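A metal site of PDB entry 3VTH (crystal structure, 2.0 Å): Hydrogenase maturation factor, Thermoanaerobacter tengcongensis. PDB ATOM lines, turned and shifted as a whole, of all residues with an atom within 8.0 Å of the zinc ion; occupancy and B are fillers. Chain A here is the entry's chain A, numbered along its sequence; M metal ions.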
ATOM      1  N   ARG A 127     -21.343   3.686  22.368  1.00  0.00           N
ATOM      2  CA  ARG A 127     -20.511   4.281  23.414  1.00  0.00           C
ATOM      3  C   ARG A 127     -21.130   5.529  24.065  1.00  0.00           C
ATOM      4  O   ARG A 127     -20.673   5.952  25.137  1.00  0.00           O
ATOM      5  CB  ARG A 127     -19.086   4.526  22.937  1.00  0.00           C
ATOM      6  CG  ARG A 127     -18.890   5.707  22.039  1.00  0.00           C
ATOM      7  CD  ARG A 127     -17.414   5.803  21.636  1.00  0.00           C
ATOM      8  NE  ARG A 127     -17.173   7.050  20.936  1.00  0.00           N
ATOM      9  CZ  ARG A 127     -16.652   8.153  21.491  1.00  0.00           C
ATOM     10  NH1 ARG A 127     -16.269   8.161  22.766  1.00  0.00           N
ATOM     11  NH2 ARG A 127     -16.506   9.236  20.759  1.00  0.00           N
ATOM     12  N   ARG A 128     -22.158   6.103  23.432  1.00  0.00           N
ATOM     13  CA  ARG A 128     -22.895   7.211  24.041  1.00  0.00           C
ATOM     14  C   ARG A 128     -24.209   6.779  24.708  1.00  0.00           C
ATOM     15  O   ARG A 128     -25.052   7.619  25.007  1.00  0.00           O
ATOM     16  CB  ARG A 128     -23.159   8.328  23.034  1.00  0.00           C
ATOM     17  CG  ARG A 128     -21.883   9.052  22.591  1.00  0.00           C
ATOM     18  CD  ARG A 128     -22.202  10.161  21.588  1.00  0.00           C
ATOM     19  NE  ARG A 128     -21.019  10.940  21.234  1.00  0.00           N
ATOM     20  CZ  ARG A 128     -20.147  10.621  20.265  1.00  0.00           C
ATOM     21  NH1 ARG A 128     -20.304   9.522  19.547  1.00  0.00           N
ATOM     22  NH2 ARG A 128     -19.116  11.428  20.026  1.00  0.00           N
ATOM     23  N   TYR A 131     -25.509   8.727  27.665  1.00  0.00           N
ATOM     24  CA  TYR A 131     -24.714   9.948  27.768  1.00  0.00           C
ATOM     25  C   TYR A 131     -25.638  11.184  27.847  1.00  0.00           C
ATOM     26  O   TYR A 131     -26.377  11.477  26.898  1.00  0.00           O
ATOM     27  CB  TYR A 131     -23.688  10.025  26.627  1.00  0.00           C
ATOM     28  CG  TYR A 131     -22.922  11.325  26.560  1.00  0.00           C
ATOM     29  CD1 TYR A 131     -22.926  12.080  25.388  1.00  0.00           C
ATOM     30  CD2 TYR A 131     -22.191  11.807  27.650  1.00  0.00           C
ATOM     31  CE1 TYR A 131     -22.203  13.272  25.302  1.00  0.00           C
ATOM     32  CE2 TYR A 131     -21.491  13.013  27.569  1.00  0.00           C
ATOM     33  CZ  TYR A 131     -21.499  13.723  26.393  1.00  0.00           C
ATOM     34  OH  TYR A 131     -20.824  14.918  26.305  1.00  0.00           O
ATOM     35  N   ARG A 153     -16.736  25.640  17.730  1.00  0.00           N
ATOM     36  CA  ARG A 153     -16.612  25.142  19.106  1.00  0.00           C
ATOM     37  C   ARG A 153     -15.909  26.144  20.042  1.00  0.00           C
ATOM     38  O   ARG A 153     -16.327  26.311  21.188  1.00  0.00           O
ATOM     39  CB  ARG A 153     -15.844  23.809  19.126  1.00  0.00           C
ATOM     40  CG  ARG A 153     -15.955  23.006  20.451  1.00  0.00           C
ATOM     41  CD  ARG A 153     -14.956  21.853  20.375  1.00  0.00           C
ATOM     42  NE  ARG A 153     -15.018  20.919  21.499  1.00  0.00           N
ATOM     43  CZ  ARG A 153     -15.728  19.789  21.506  1.00  0.00           C
ATOM     44  NH1 ARG A 153     -16.504  19.467  20.464  1.00  0.00           N
ATOM     45  NH2 ARG A 153     -15.662  18.982  22.556  1.00  0.00           N
ATOM     46  N   PHE A 161     -13.949  22.082  26.845  1.00  0.00           N
ATOM     47  CA  PHE A 161     -14.043  20.623  26.738  1.00  0.00           C
ATOM     48  C   PHE A 161     -13.337  20.126  25.471  1.00  0.00           C
ATOM     49  O   PHE A 161     -14.009  19.772  24.501  1.00  0.00           O
ATOM     50  CB  PHE A 161     -15.514  20.202  26.710  1.00  0.00           C
ATOM     51  CG  PHE A 161     -16.233  20.429  28.011  1.00  0.00           C
ATOM     52  CD1 PHE A 161     -16.064  19.547  29.093  1.00  0.00           C
ATOM     53  CD2 PHE A 161     -17.093  21.529  28.152  1.00  0.00           C
ATOM     54  CE1 PHE A 161     -16.724  19.762  30.303  1.00  0.00           C
ATOM     55  CE2 PHE A 161     -17.762  21.742  29.367  1.00  0.00           C
ATOM     56  CZ  PHE A 161     -17.588  20.858  30.435  1.00  0.00           C
ATOM     57  N   PRO A 162     -12.002  20.083  25.457  1.00  0.00           N
ATOM     58  CA  PRO A 162     -11.321  19.582  24.250  1.00  0.00           C
ATOM     59  C   PRO A 162     -11.685  18.128  23.945  1.00  0.00           C
ATOM     60  O   PRO A 162     -11.816  17.315  24.863  1.00  0.00           O
ATOM     61  CB  PRO A 162      -9.829  19.708  24.600  1.00  0.00           C
ATOM     62  CG  PRO A 162      -9.774  19.721  26.066  1.00  0.00           C
ATOM     63  CD  PRO A 162     -11.034  20.427  26.522  1.00  0.00           C
ATOM     64  N   MET A 163     -11.862  17.821  22.666  1.00  0.00           N
ATOM     65  CA  MET A 163     -12.297  16.486  22.238  1.00  0.00           C
ATOM     66  C   MET A 163     -11.243  15.449  22.593  1.00  0.00           C
ATOM     67  O   MET A 163     -10.040  15.682  22.431  1.00  0.00           O
ATOM     68  CB  MET A 163     -12.479  16.422  20.709  1.00  0.00           C
ATOM     69  CG  MET A 163     -13.576  17.265  20.126  1.00  0.00           C
ATOM     70  SD  MET A 163     -13.543  17.128  18.298  1.00  0.00           S
ATOM     71  CE  MET A 163     -12.004  17.952  17.872  1.00  0.00           C
ATOM     72  N   CYS A 164     -11.713  14.290  23.055  1.00  0.00           N
ATOM     73  CA  CYS A 164     -10.854  13.115  23.226  1.00  0.00           C
ATOM     74  C   CYS A 164     -10.481  12.558  21.852  1.00  0.00           C
ATOM     75  O   CYS A 164     -11.036  12.963  20.822  1.00  0.00           O
ATOM     76  CB  CYS A 164     -11.580  12.040  24.048  1.00  0.00           C
ATOM     77  SG  CYS A 164     -12.952  11.232  23.154  1.00  0.00           S
ATOM     78  N   GLU A 165      -9.529  11.624  21.847  1.00  0.00           N
ATOM     79  CA  GLU A 165      -9.041  10.985  20.631  1.00  0.00           C
ATOM     80  C   GLU A 165     -10.169  10.338  19.808  1.00  0.00           C
ATOM     81  O   GLU A 165     -10.167  10.426  18.579  1.00  0.00           O
ATOM     82  CB  GLU A 165      -7.961   9.954  20.972  1.00  0.00           C
ATOM     83  CG  GLU A 165      -7.270   9.308  19.785  1.00  0.00           C
ATOM     84  CD  GLU A 165      -6.219   8.269  20.177  1.00  0.00           C
ATOM     85  OE1 GLU A 165      -6.276   7.695  21.291  1.00  0.00           O
ATOM     86  OE2 GLU A 165      -5.306   8.012  19.352  1.00  0.00           O
ATOM     87  N   LYS A 166     -11.121   9.701  20.480  1.00  0.00           N
ATOM     88  CA  LYS A 166     -12.227   9.055  19.764  1.00  0.00           C
ATOM     89  C   LYS A 166     -13.178  10.055  19.110  1.00  0.00           C
ATOM     90  O   LYS A 166     -13.623   9.871  17.969  1.00  0.00           O
ATOM     91  CB  LYS A 166     -13.014   8.124  20.682  1.00  0.00           C
ATOM     92  CG  LYS A 166     -12.285   6.851  21.044  1.00  0.00           C
ATOM     93  CD  LYS A 166     -13.300   5.795  21.485  1.00  0.00           C
ATOM     94  CE  LYS A 166     -13.496   5.769  22.984  1.00  0.00           C
ATOM     95  NZ  LYS A 166     -12.462   4.866  23.597  1.00  0.00           N
ATOM     96  N   CYS A 167     -13.499  11.123  19.831  1.00  0.00           N
ATOM     97  CA  CYS A 167     -14.403  12.148  19.297  1.00  0.00           C
ATOM     98  C   CYS A 167     -13.745  12.886  18.142  1.00  0.00           C
ATOM     99  O   CYS A 167     -14.406  13.222  17.164  1.00  0.00           O
ATOM    100  CB  CYS A 167     -14.839  13.125  20.387  1.00  0.00           C
ATOM    101  SG  CYS A 167     -16.062  12.397  21.486  1.00  0.00           S
ATOM    102  N   SER A 168     -12.444  13.140  18.278  1.00  0.00           N
ATOM    103  CA  SER A 168     -11.656  13.773  17.213  1.00  0.00           C
ATOM    104  C   SER A 168     -11.581  12.925  15.938  1.00  0.00           C
ATOM    105  O   SER A 168     -11.624  13.460  14.814  1.00  0.00           O
ATOM    106  CB  SER A 168     -10.249  14.070  17.716  1.00  0.00           C
ATOM    107  OG  SER A 168      -9.487  14.660  16.692  1.00  0.00           O
ATOM    108  N   GLU A 170     -13.978  10.785  15.006  1.00  0.00           N
ATOM    109  CA  GLU A 170     -15.313  10.947  14.445  1.00  0.00           C
ATOM    110  C   GLU A 170     -15.445  12.279  13.711  1.00  0.00           C
ATOM    111  O   GLU A 170     -15.972  12.343  12.587  1.00  0.00           O
ATOM    112  CB  GLU A 170     -16.375  10.891  15.547  1.00  0.00           C
ATOM    113  CG  GLU A 170     -16.564   9.530  16.189  1.00  0.00           C
ATOM    114  CD  GLU A 170     -17.630   9.579  17.285  1.00  0.00           C
ATOM    115  OE1 GLU A 170     -17.689  10.593  18.017  1.00  0.00           O
ATOM    116  OE2 GLU A 170     -18.418   8.627  17.418  1.00  0.00           O
ATOM    117  N   VAL A 184     -19.351  17.998  19.199  1.00  0.00           N
ATOM    118  CA  VAL A 184     -19.082  16.570  19.478  1.00  0.00           C
ATOM    119  C   VAL A 184     -18.326  16.334  20.805  1.00  0.00           C
ATOM    120  O   VAL A 184     -17.272  16.938  21.083  1.00  0.00           O
ATOM    121  CB  VAL A 184     -18.351  15.864  18.298  1.00  0.00           C
ATOM    122  CG1 VAL A 184     -16.963  16.453  18.071  1.00  0.00           C
ATOM    123  CG2 VAL A 184     -18.257  14.351  18.538  1.00  0.00           C
ATOM    124  N   ALA A 185     -18.870  15.446  21.633  1.00  0.00           N
ATOM    125  CA  ALA A 185     -18.275  15.084  22.908  1.00  0.00           C
ATOM    126  C   ALA A 185     -18.831  13.748  23.353  1.00  0.00           C
ATOM    127  O   ALA A 185     -19.756  13.228  22.703  1.00  0.00           O
ATOM    128  CB  ALA A 185     -18.564  16.162  23.973  1.00  0.00           C
ATOM    129  N   CYS A 186     -18.302  13.220  24.456  1.00  0.00           N
ATOM    130  CA  CYS A 186     -18.704  11.898  24.955  1.00  0.00           C
ATOM    131  C   CYS A 186     -18.501  11.835  26.468  1.00  0.00           C
ATOM    132  O   CYS A 186     -18.167  12.843  27.087  1.00  0.00           O
ATOM    133  CB  CYS A 186     -17.875  10.804  24.265  1.00  0.00           C
ATOM    134  SG  CYS A 186     -16.128  10.708  24.802  1.00  0.00           S
ATOM    135  N   PHE A 187     -18.714  10.659  27.057  1.00  0.00           N
ATOM    136  CA  PHE A 187     -18.480  10.461  28.507  1.00  0.00           C
ATOM    137  C   PHE A 187     -17.089  10.933  28.946  1.00  0.00           C
ATOM    138  O   PHE A 187     -16.928  11.520  30.012  1.00  0.00           O
ATOM    139  CB  PHE A 187     -18.657   8.989  28.909  1.00  0.00           C
ATOM    140  CG  PHE A 187     -20.088   8.610  29.209  1.00  0.00           C
ATOM    141  CD1 PHE A 187     -20.745   9.141  30.323  1.00  0.00           C
ATOM    142  CD2 PHE A 187     -20.774   7.721  28.394  1.00  0.00           C
ATOM    143  CE1 PHE A 187     -22.059   8.792  30.617  1.00  0.00           C
ATOM    144  CE2 PHE A 187     -22.104   7.375  28.682  1.00  0.00           C
ATOM    145  CZ  PHE A 187     -22.738   7.892  29.792  1.00  0.00           C
ATOM    146  N   ASP A 188     -16.094  10.668  28.099  1.00  0.00           N
ATOM    147  CA  ASP A 188     -14.677  10.896  28.440  1.00  0.00           C
ATOM    148  C   ASP A 188     -14.241  12.358  28.323  1.00  0.00           C
ATOM    149  O   ASP A 188     -13.333  12.800  29.036  1.00  0.00           O
ATOM    150  CB  ASP A 188     -13.789  10.041  27.531  1.00  0.00           C
ATOM    151  CG  ASP A 188     -14.039   8.539  27.698  1.00  0.00           C
ATOM    152  OD1 ASP A 188     -13.880   7.792  26.706  1.00  0.00           O
ATOM    153  OD2 ASP A 188     -14.410   8.100  28.802  1.00  0.00           O
ATOM    154  N   CYS A 189     -14.856  13.122  27.419  1.00  0.00           N
ATOM    155  CA  CYS A 189     -14.360  14.469  27.148  1.00  0.00           C
ATOM    156  C   CYS A 189     -15.442  15.532  27.333  1.00  0.00           C
ATOM    157  O   CYS A 189     -15.160  16.734  27.228  1.00  0.00           O
ATOM    158  CB  CYS A 189     -13.761  14.541  25.731  1.00  0.00           C
ATOM    159  SG  CYS A 189     -14.966  14.419  24.364  1.00  0.00           S
ATOM    160  N   GLY A 190     -16.663  15.093  27.611  1.00  0.00           N
ATOM    161  CA  GLY A 190     -17.804  15.997  27.641  1.00  0.00           C
ATOM    162  C   GLY A 190     -18.141  16.496  29.035  1.00  0.00           C
ATOM    163  O   GLY A 190     -17.498  16.130  30.010  1.00  0.00           O
HETATM  164 ZN    ZN M   1     -14.995  12.264  23.521  1.00  0.00          ZN
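The side-chain sulfur of Cys 164 sits close to the backbone NH of Lys 166, at 3.6 Å.
SG of Cys 186 lies close to N of Asp 188 (3.3 Å).
The side-chain sulfur (SG) of Cys 167 sits close to the guanidinium group (NH2) of Arg 128 (3.5 Å).
SG of Cys 186 lies close to NH1 of Arg 127 (3.3 Å).
The side-chain sulfur (SG) of Cys 167 lies close to the guanidinium group (NH2) of Arg 127.
O of Cys 186 lies close to OH of Tyr 131.
Within 4 Å of the zinc ion: Cys 164, Cys 167, Cys 186 and Cys 189.
Along chain A the residues within 4 Å of the zinc ion span positions 164 to 189.
The nearest printed residue that does not touch the zinc ion is Ala 185 (4.1 Å).
The zinc ion is bound by SG of Cys 167, SG of Cys 186, SG of Cys 189 and SG of Cys 164.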
